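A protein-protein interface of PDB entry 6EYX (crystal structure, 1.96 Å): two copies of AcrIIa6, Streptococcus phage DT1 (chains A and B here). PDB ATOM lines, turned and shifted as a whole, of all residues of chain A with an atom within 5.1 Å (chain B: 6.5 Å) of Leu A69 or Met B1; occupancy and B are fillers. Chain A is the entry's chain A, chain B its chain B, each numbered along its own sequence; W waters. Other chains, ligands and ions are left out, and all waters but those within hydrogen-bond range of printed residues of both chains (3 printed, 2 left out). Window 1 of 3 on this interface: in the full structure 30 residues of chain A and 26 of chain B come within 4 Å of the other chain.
N of Met A1 sits at hydrogen-bond distance from OD1 of Asp B66 (2.9 Å). The side-chain amide oxygen (OD1) of Asn A57 is in hydrogen-bond range of the side-chain amide nitrogen (ND2) of Asn B57. The side-chain carboxylate (OD1) of Asp A61 lies within hydrogen-bond range of the backbone NH (N) of Met B1, at 2.8 Å. OD1 of Asp A65 is in salt-bridge range of NZ of Lys B74 (2.8 Å). The side-chain carboxylate of Asp A66 is in hydrogen-bond range of the backbone NH of Met B1 (2.8 Å).
The side-chain carboxylate of Asp A65 is in hydrogen-bond range of the backbone NH of Phe A67, at 2.8 Å. The side-chain carboxylate of Glu A68 sits at hydrogen-bond distance from the backbone NH of Asp A65, 3.0 Å away.
Among the printed residues, merely in contact across the chains: Asn A57 with Met B1 (3.9 Å), Asn A57 with Ile B3 (3.5 Å), Asp A66 with Ala B70 (3.2 Å), Asp A66 with Gly B73 (3.4 Å), Asp A66 with Lys B74 (3.7 Å), Phe A67 with Ala B70 (3.9 Å), Leu A69 with Met B1 (3.9 Å), Ala A70 with Asp B66 (3.2 Å), Ala A70 with Ala B70 (3.8 Å) and Gly A73 with Asp B66 (3.4 Å).
Of the printed residues of chain B, Asp A65 touches Lys B74. Leu A69 touches just one residue of chain B: Met B1 (3.9 Å). Met B1 touches just these residues of chain A: Asn A57, Asp A61, Asp A66 and Leu A69. Of the printed residues of chain A, Ile B3 touches Asn A57 (3.5 Å). Leu B60 touches none of the printed residues of chain A. The nearest residue of chain B that does not touch Leu A69 is Asp B66 (4.8 Å). The nearest printed residue of chain A that does not touch Met B1 is Leu A60 (5.9 Å). The nearest printed residue of chain B that does not touch Phe A67 is Lys B74 (4.1 Å).
Of the 13 printed residues of chain B, 7 touch a printed residue of chain A. Printed residues of chain B that touch a printed residue of chain A: Met B1, Ile B3, Asn B57, Asp B66, Ala B70, Gly B73 and Lys B74. Of the 14 printed residues of chain A, 9 touch a printed residue of chain B. Hydrophobic or aromatic side chains of chain A within 4 Å of the printed part of chain B: Met A1, Leu A69 and Ala A70.
Met A1 touches Asp B66, and with the chains exchanged Asp A66 touches Met B1. Asn A57 touches its own counterpart, Asn B57. Asp A66 touches Gly B73, and with the chains exchanged Gly A73 touches Asp B66. Leu A69 touches Met B1, but with the chains exchanged Met A1 does not touch Leu B69 (4.3 Å).
Water W2 bridges the side-chain carboxylate (OD2) of Asp B66 (2.7 Å) and the backbone NH (N) of Met A1 (2.8 Å). Water W3 bridges O of Asn A57 (2.8 Å) and N of Met B1 (2.9 Å). Water W1 lies within hydrogen-bond range of the side-chain amino group of Lys B74 (2.9 Å), the backbone NH of Asp A66 (3.0 Å) and the side-chain carboxylate of Asp A65 (3.4 Å).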
ATOM      1  N   MET A   1     -12.990  -7.669   8.335  1.00  0.00           N
ATOM      2  CA  MET A   1     -13.580  -7.748   9.663  1.00  0.00           C
ATOM      3  C   MET A   1     -12.920  -8.823  10.522  1.00  0.00           C
ATOM      4  O   MET A   1     -12.691  -9.937  10.049  1.00  0.00           O
ATOM      5  CB  MET A   1     -15.072  -8.003   9.544  1.00  0.00           C
ATOM      6  CG  MET A   1     -15.759  -8.294  10.855  1.00  0.00           C
ATOM      7  SD  MET A   1     -17.339  -7.458  10.942  1.00  0.00           S
ATOM      8  CE  MET A   1     -16.932  -6.191  12.087  1.00  0.00           C
ATOM      9  N   ASN A  57     -22.687 -11.621  16.620  1.00  0.00           N
ATOM     10  CA  ASN A  57     -23.213 -10.963  15.427  1.00  0.00           C
ATOM     11  C   ASN A  57     -24.607 -10.367  15.641  1.00  0.00           C
ATOM     12  O   ASN A  57     -24.936  -9.389  14.976  1.00  0.00           O
ATOM     13  CB  ASN A  57     -23.137 -11.880  14.206  1.00  0.00           C
ATOM     14  CG  ASN A  57     -21.702 -12.064  13.751  1.00  0.00           C
ATOM     15  OD1 ASN A  57     -21.001 -12.973  14.187  1.00  0.00           O
ATOM     16  ND2 ASN A  57     -21.196 -11.152  12.943  1.00  0.00           N
ATOM     17  N   LEU A  60     -23.896  -6.954  17.164  1.00  0.00           N
ATOM     18  CA  LEU A  60     -23.466  -6.073  16.075  1.00  0.00           C
ATOM     19  C   LEU A  60     -24.621  -5.674  15.185  1.00  0.00           C
ATOM     20  O   LEU A  60     -24.736  -4.497  14.830  1.00  0.00           O
ATOM     21  CB  LEU A  60     -22.340  -6.727  15.258  1.00  0.00           C
ATOM     22  CG  LEU A  60     -20.996  -6.862  15.945  1.00  0.00           C
ATOM     23  CD1 LEU A  60     -20.080  -7.797  15.152  1.00  0.00           C
ATOM     24  CD2 LEU A  60     -20.330  -5.500  16.147  1.00  0.00           C
ATOM     25  N   ASP A  61     -25.518  -6.635  14.853  1.00  0.00           N
ATOM     26  CA  ASP A  61     -26.697  -6.412  14.007  1.00  0.00           C
ATOM     27  C   ASP A  61     -27.659  -5.387  14.619  1.00  0.00           C
ATOM     28  O   ASP A  61     -28.212  -4.552  13.894  1.00  0.00           O
ATOM     29  CB  ASP A  61     -27.424  -7.730  13.698  1.00  0.00           C
ATOM     30  CG  ASP A  61     -28.598  -7.550  12.751  1.00  0.00           C
ATOM     31  OD1 ASP A  61     -28.362  -7.182  11.578  1.00  0.00           O
ATOM     32  OD2 ASP A  61     -29.751  -7.732  13.197  1.00  0.00           O
ATOM     33  N   PHE A  64     -25.506  -1.712  14.710  1.00  0.00           N
ATOM     34  CA  PHE A  64     -25.024  -1.164  13.437  1.00  0.00           C
ATOM     35  C   PHE A  64     -25.837  -1.586  12.235  1.00  0.00           C
ATOM     36  O   PHE A  64     -26.237  -2.747  12.109  1.00  0.00           O
ATOM     37  CB  PHE A  64     -23.553  -1.584  13.208  1.00  0.00           C
ATOM     38  CG  PHE A  64     -22.625  -1.167  14.329  1.00  0.00           C
ATOM     39  CD1 PHE A  64     -22.138   0.134  14.401  1.00  0.00           C
ATOM     40  CD2 PHE A  64     -22.269  -2.065  15.335  1.00  0.00           C
ATOM     41  CE1 PHE A  64     -21.321   0.539  15.470  1.00  0.00           C
ATOM     42  CE2 PHE A  64     -21.449  -1.663  16.397  1.00  0.00           C
ATOM     43  CZ  PHE A  64     -20.985  -0.368  16.459  1.00  0.00           C
ATOM     44  N   ASP A  65     -25.984  -0.655  11.288  1.00  0.00           N
ATOM     45  CA  ASP A  65     -26.566  -0.947   9.989  1.00  0.00           C
ATOM     46  C   ASP A  65     -25.558  -1.881   9.309  1.00  0.00           C
ATOM     47  O   ASP A  65     -24.360  -1.815   9.619  1.00  0.00           O
ATOM     48  CB  ASP A  65     -26.687   0.342   9.166  1.00  0.00           C
ATOM     49  CG  ASP A  65     -27.400   0.145   7.845  1.00  0.00           C
ATOM     50  OD1 ASP A  65     -26.729  -0.251   6.854  1.00  0.00           O
ATOM     51  OD2 ASP A  65     -28.607   0.438   7.782  1.00  0.00           O
ATOM     52  N   ASP A  66     -26.027  -2.754   8.408  1.00  0.00           N
ATOM     53  CA  ASP A  66     -25.137  -3.665   7.670  1.00  0.00           C
ATOM     54  C   ASP A  66     -24.038  -2.900   6.924  1.00  0.00           C
ATOM     55  O   ASP A  66     -22.916  -3.373   6.890  1.00  0.00           O
ATOM     56  CB  ASP A  66     -25.919  -4.580   6.717  1.00  0.00           C
ATOM     57  CG  ASP A  66     -26.593  -5.727   7.452  1.00  0.00           C
ATOM     58  OD1 ASP A  66     -25.870  -6.556   8.051  1.00  0.00           O
ATOM     59  OD2 ASP A  66     -27.834  -5.771   7.457  1.00  0.00           O
ATOM     60  N   PHE A  67     -24.335  -1.707   6.408  1.00  0.00           N
ATOM     61  CA  PHE A  67     -23.287  -0.904   5.740  1.00  0.00           C
ATOM     62  C   PHE A  67     -22.229  -0.431   6.769  1.00  0.00           C
ATOM     63  O   PHE A  67     -21.039  -0.377   6.447  1.00  0.00           O
ATOM     64  CB  PHE A  67     -23.878   0.271   4.948  1.00  0.00           C
ATOM     65  CG  PHE A  67     -22.811   1.130   4.304  1.00  0.00           C
ATOM     66  CD1 PHE A  67     -22.093   0.669   3.200  1.00  0.00           C
ATOM     67  CD2 PHE A  67     -22.479   2.373   4.837  1.00  0.00           C
ATOM     68  CE1 PHE A  67     -21.067   1.441   2.640  1.00  0.00           C
ATOM     69  CE2 PHE A  67     -21.462   3.150   4.267  1.00  0.00           C
ATOM     70  CZ  PHE A  67     -20.772   2.682   3.165  1.00  0.00           C
ATOM     71  N   GLU A  68     -22.656  -0.145   8.016  1.00  0.00           N
ATOM     72  CA  GLU A  68     -21.742   0.269   9.086  1.00  0.00           C
ATOM     73  C   GLU A  68     -20.837  -0.901   9.477  1.00  0.00           C
ATOM     74  O   GLU A  68     -19.663  -0.688   9.783  1.00  0.00           O
ATOM     75  CB  GLU A  68     -22.506   0.804  10.302  1.00  0.00           C
ATOM     76  CG  GLU A  68     -23.208   2.134  10.042  1.00  0.00           C
ATOM     77  CD  GLU A  68     -23.879   2.704  11.273  1.00  0.00           C
ATOM     78  OE1 GLU A  68     -24.610   1.958  11.959  1.00  0.00           O
ATOM     79  OE2 GLU A  68     -23.678   3.907  11.550  1.00  0.00           O
ATOM     80  N   LEU A  69     -21.355  -2.137   9.372  1.00  0.00           N
ATOM     81  CA  LEU A  69     -20.559  -3.351   9.619  1.00  0.00           C
ATOM     82  C   LEU A  69     -19.426  -3.474   8.587  1.00  0.00           C
ATOM     83  O   LEU A  69     -18.313  -3.855   8.944  1.00  0.00           O
ATOM     84  CB  LEU A  69     -21.453  -4.592   9.637  1.00  0.00           C
ATOM     85  CG  LEU A  69     -22.439  -4.652  10.821  1.00  0.00           C
ATOM     86  CD1 LEU A  69     -23.355  -5.844  10.700  1.00  0.00           C
ATOM     87  CD2 LEU A  69     -21.699  -4.693  12.159  1.00  0.00           C
ATOM     88  N   ALA A  70     -19.684  -3.045   7.337  1.00  0.00           N
ATOM     89  CA  ALA A  70     -18.639  -3.021   6.296  1.00  0.00           C
ATOM     90  C   ALA A  70     -17.610  -1.928   6.647  1.00  0.00           C
ATOM     91  O   ALA A  70     -16.412  -2.174   6.529  1.00  0.00           O
ATOM     92  CB  ALA A  70     -19.247  -2.756   4.919  1.00  0.00           C
ATOM     93  N   MET A  71     -18.080  -0.736   7.104  1.00  0.00           N
ATOM     94  CA  MET A  71     -17.197   0.372   7.512  1.00  0.00           C
ATOM     95  C   MET A  71     -16.300  -0.036   8.684  1.00  0.00           C
ATOM     96  O   MET A  71     -15.128   0.324   8.692  1.00  0.00           O
ATOM     97  CB  MET A  71     -17.986   1.640   7.868  1.00  0.00           C
ATOM     98  CG  MET A  71     -18.588   2.338   6.671  1.00  0.00           C
ATOM     99  SD  MET A  71     -19.033   4.073   7.005  1.00  0.00           S
ATOM    100  CE  MET A  71     -20.382   3.853   8.163  1.00  0.00           C
ATOM    101  N   ILE A  72     -16.827  -0.822   9.640  1.00  0.00           N
ATOM    102  CA  ILE A  72     -16.031  -1.318  10.768  1.00  0.00           C
ATOM    103  C   ILE A  72     -14.839  -2.142  10.252  1.00  0.00           C
ATOM    104  O   ILE A  72     -13.718  -1.929  10.704  1.00  0.00           O
ATOM    105  CB  ILE A  72     -16.894  -2.105  11.800  1.00  0.00           C
ATOM    106  CG1 ILE A  72     -17.919  -1.176  12.494  1.00  0.00           C
ATOM    107  CG2 ILE A  72     -16.003  -2.759  12.848  1.00  0.00           C
ATOM    108  CD1 ILE A  72     -19.144  -1.907  13.161  1.00  0.00           C
ATOM    109  N   GLY A  73     -15.099  -3.073   9.328  1.00  0.00           N
ATOM    110  CA  GLY A  73     -14.066  -3.920   8.740  1.00  0.00           C
ATOM    111  C   GLY A  73     -13.024  -3.140   7.960  1.00  0.00           C
ATOM    112  O   GLY A  73     -11.822  -3.389   8.097  1.00  0.00           O
ATOM    113  N   MET B   1     -26.248  -8.335  10.158  1.00  0.00           N
ATOM    114  CA  MET B   1     -26.597  -9.622   9.570  1.00  0.00           C
ATOM    115  C   MET B   1     -26.981 -10.668  10.644  1.00  0.00           C
ATOM    116  O   MET B   1     -27.114 -10.304  11.814  1.00  0.00           O
ATOM    117  CB  MET B   1     -25.456 -10.122   8.661  1.00  0.00           C
ATOM    118  CG  MET B   1     -24.100 -10.281   9.350  1.00  0.00           C
ATOM    119  SD  MET B   1     -22.962 -11.195   8.287  1.00  0.00           S
ATOM    120  CE  MET B   1     -23.643 -12.849   8.423  1.00  0.00           C
ATOM    121  N   LYS B   2     -27.173 -11.951  10.251  1.00  0.00           N
ATOM    122  CA  LYS B   2     -27.526 -13.015  11.187  1.00  0.00           C
ATOM    123  C   LYS B   2     -26.750 -14.302  10.908  1.00  0.00           C
ATOM    124  O   LYS B   2     -26.773 -14.784   9.776  1.00  0.00           O
ATOM    125  CB  LYS B   2     -29.040 -13.281  11.158  1.00  0.00           C
ATOM    126  CG  LYS B   2     -29.488 -14.259  12.220  1.00  0.00           C
ATOM    127  CD  LYS B   2     -30.976 -14.468  12.197  1.00  0.00           C
ATOM    128  CE  LYS B   2     -31.482 -14.632  13.601  1.00  0.00           C
ATOM    129  NZ  LYS B   2     -32.899 -15.068  13.621  1.00  0.00           N
ATOM    130  N   ILE B   3     -26.106 -14.882  11.945  1.00  0.00           N
ATOM    131  CA  ILE B   3     -25.375 -16.143  11.790  1.00  0.00           C
ATOM    132  C   ILE B   3     -26.360 -17.303  11.991  1.00  0.00           C
ATOM    133  O   ILE B   3     -26.964 -17.417  13.057  1.00  0.00           O
ATOM    134  CB  ILE B   3     -24.123 -16.249  12.722  1.00  0.00           C
ATOM    135  CG1 ILE B   3     -23.081 -15.129  12.421  1.00  0.00           C
ATOM    136  CG2 ILE B   3     -23.499 -17.663  12.695  1.00  0.00           C
ATOM    137  CD1 ILE B   3     -22.337 -15.139  11.074  1.00  0.00           C
ATOM    138  N   ILE B   7     -25.933 -19.116   6.372  1.00  0.00           N
ATOM    139  CA  ILE B   7     -24.565 -18.581   6.307  1.00  0.00           C
ATOM    140  C   ILE B   7     -23.559 -19.712   6.173  1.00  0.00           C
ATOM    141  O   ILE B   7     -22.591 -19.587   5.415  1.00  0.00           O
ATOM    142  CB  ILE B   7     -24.271 -17.604   7.491  1.00  0.00           C
ATOM    143  CG1 ILE B   7     -25.215 -16.371   7.462  1.00  0.00           C
ATOM    144  CG2 ILE B   7     -22.796 -17.184   7.575  1.00  0.00           C
ATOM    145  CD1 ILE B   7     -25.220 -15.509   6.207  1.00  0.00           C
ATOM    146  N   ASN B  57     -16.249 -15.495  11.802  1.00  0.00           N
ATOM    147  CA  ASN B  57     -15.978 -14.239  11.121  1.00  0.00           C
ATOM    148  C   ASN B  57     -14.671 -14.285  10.315  1.00  0.00           C
ATOM    149  O   ASN B  57     -14.584 -13.576   9.315  1.00  0.00           O
ATOM    150  CB  ASN B  57     -16.064 -13.044  12.074  1.00  0.00           C
ATOM    151  CG  ASN B  57     -17.502 -12.754  12.465  1.00  0.00           C
ATOM    152  OD1 ASN B  57     -18.226 -12.041  11.780  1.00  0.00           O
ATOM    153  ND2 ASN B  57     -18.004 -13.403  13.494  1.00  0.00           N
ATOM    154  N   LEU B  60     -15.709 -15.845   7.013  1.00  0.00           N
ATOM    155  CA  LEU B  60     -16.415 -14.811   6.243  1.00  0.00           C
ATOM    156  C   LEU B  60     -15.459 -13.752   5.696  1.00  0.00           C
ATOM    157  O   LEU B  60     -15.573 -13.386   4.530  1.00  0.00           O
ATOM    158  CB  LEU B  60     -17.517 -14.160   7.086  1.00  0.00           C
ATOM    159  CG  LEU B  60     -18.728 -15.032   7.398  1.00  0.00           C
ATOM    160  CD1 LEU B  60     -19.578 -14.390   8.482  1.00  0.00           C
ATOM    161  CD2 LEU B  60     -19.549 -15.316   6.140  1.00  0.00           C
ATOM    162  N   ASP B  66     -15.399  -6.808   2.813  1.00  0.00           N
ATOM    163  CA  ASP B  66     -16.243  -6.209   3.858  1.00  0.00           C
ATOM    164  C   ASP B  66     -17.529  -5.613   3.272  1.00  0.00           C
ATOM    165  O   ASP B  66     -18.567  -5.722   3.900  1.00  0.00           O
ATOM    166  CB  ASP B  66     -15.486  -5.166   4.692  1.00  0.00           C
ATOM    167  CG  ASP B  66     -14.560  -5.793   5.717  1.00  0.00           C
ATOM    168  OD1 ASP B  66     -15.060  -6.498   6.617  1.00  0.00           O
ATOM    169  OD2 ASP B  66     -13.343  -5.604   5.603  1.00  0.00           O
ATOM    170  N   LEU B  69     -19.952  -8.380   2.851  1.00  0.00           N
ATOM    171  CA  LEU B  69     -20.519  -8.742   4.157  1.00  0.00           C
ATOM    172  C   LEU B  69     -21.746  -7.878   4.464  1.00  0.00           C
ATOM    173  O   LEU B  69     -22.733  -8.387   5.003  1.00  0.00           O
ATOM    174  CB  LEU B  69     -19.463  -8.651   5.258  1.00  0.00           C
ATOM    175  CG  LEU B  69     -18.327  -9.701   5.152  1.00  0.00           C
ATOM    176  CD1 LEU B  69     -17.271  -9.461   6.203  1.00  0.00           C
ATOM    177  CD2 LEU B  69     -18.870 -11.132   5.272  1.00  0.00           C
ATOM    178  N   ALA B  70     -21.720  -6.591   4.043  1.00  0.00           N
ATOM    179  CA  ALA B  70     -22.889  -5.706   4.181  1.00  0.00           C
ATOM    180  C   ALA B  70     -24.004  -6.199   3.243  1.00  0.00           C
ATOM    181  O   ALA B  70     -25.154  -6.245   3.666  1.00  0.00           O
ATOM    182  CB  ALA B  70     -22.521  -4.267   3.858  1.00  0.00           C
ATOM    183  N   ILE B  72     -24.545  -9.264   2.197  1.00  0.00           N
ATOM    184  CA  ILE B  72     -25.110 -10.486   2.775  1.00  0.00           C
ATOM    185  C   ILE B  72     -26.219 -10.135   3.771  1.00  0.00           C
ATOM    186  O   ILE B  72     -27.286 -10.735   3.711  1.00  0.00           O
ATOM    187  CB  ILE B  72     -24.015 -11.395   3.416  1.00  0.00           C
ATOM    188  CG1 ILE B  72     -23.049 -11.945   2.348  1.00  0.00           C
ATOM    189  CG2 ILE B  72     -24.652 -12.561   4.185  1.00  0.00           C
ATOM    190  CD1 ILE B  72     -21.659 -12.444   2.892  1.00  0.00           C
ATOM    191  N   GLY B  73     -25.945  -9.191   4.683  1.00  0.00           N
ATOM    192  CA  GLY B  73     -26.909  -8.746   5.684  1.00  0.00           C
ATOM    193  C   GLY B  73     -28.142  -8.106   5.074  1.00  0.00           C
ATOM    194  O   GLY B  73     -29.258  -8.398   5.492  1.00  0.00           O
ATOM    195  N   LYS B  74     -27.955  -7.238   4.070  1.00  0.00           N
ATOM    196  CA  LYS B  74     -29.081  -6.585   3.373  1.00  0.00           C
ATOM    197  C   LYS B  74     -29.909  -7.655   2.604  1.00  0.00           C
ATOM    198  O   LYS B  74     -31.147  -7.615   2.647  1.00  0.00           O
ATOM    199  CB  LYS B  74     -28.574  -5.498   2.395  1.00  0.00           C
ATOM    200  CG  LYS B  74     -27.786  -4.353   3.043  1.00  0.00           C
ATOM    201  CD  LYS B  74     -28.661  -3.334   3.739  1.00  0.00           C
ATOM    202  CE  LYS B  74     -27.821  -2.264   4.389  1.00  0.00           C
ATOM    203  NZ  LYS B  74     -28.681  -1.331   5.163  1.00  0.00           N
ATOM    204  N   GLN B  76     -30.188 -10.869   3.373  1.00  0.00           N
ATOM    205  CA  GLN B  76     -30.896 -11.622   4.427  1.00  0.00           C
ATOM    206  C   GLN B  76     -32.213 -10.945   4.815  1.00  0.00           C
ATOM    207  O   GLN B  76     -33.240 -11.626   4.917  1.00  0.00           O
ATOM    208  CB  GLN B  76     -30.000 -11.804   5.656  1.00  0.00           C
ATOM    209  CG  GLN B  76     -29.061 -12.994   5.561  1.00  0.00           C
ATOM    210  CD  GLN B  76     -28.319 -13.230   6.854  1.00  0.00           C
ATOM    211  OE1 GLN B  76     -27.638 -12.344   7.366  1.00  0.00           O
ATOM    212  NE2 GLN B  76     -28.420 -14.434   7.401  1.00  0.00           N
HETATM  213  O   HOH W   1     -28.886  -2.955   7.541  1.00  0.00           O
HETATM  214  O   HOH W   2     -11.149  -7.094   6.288  1.00  0.00           O
HETATM  215  O   HOH W   3     -24.308  -8.767  12.329  1.00  0.00           O
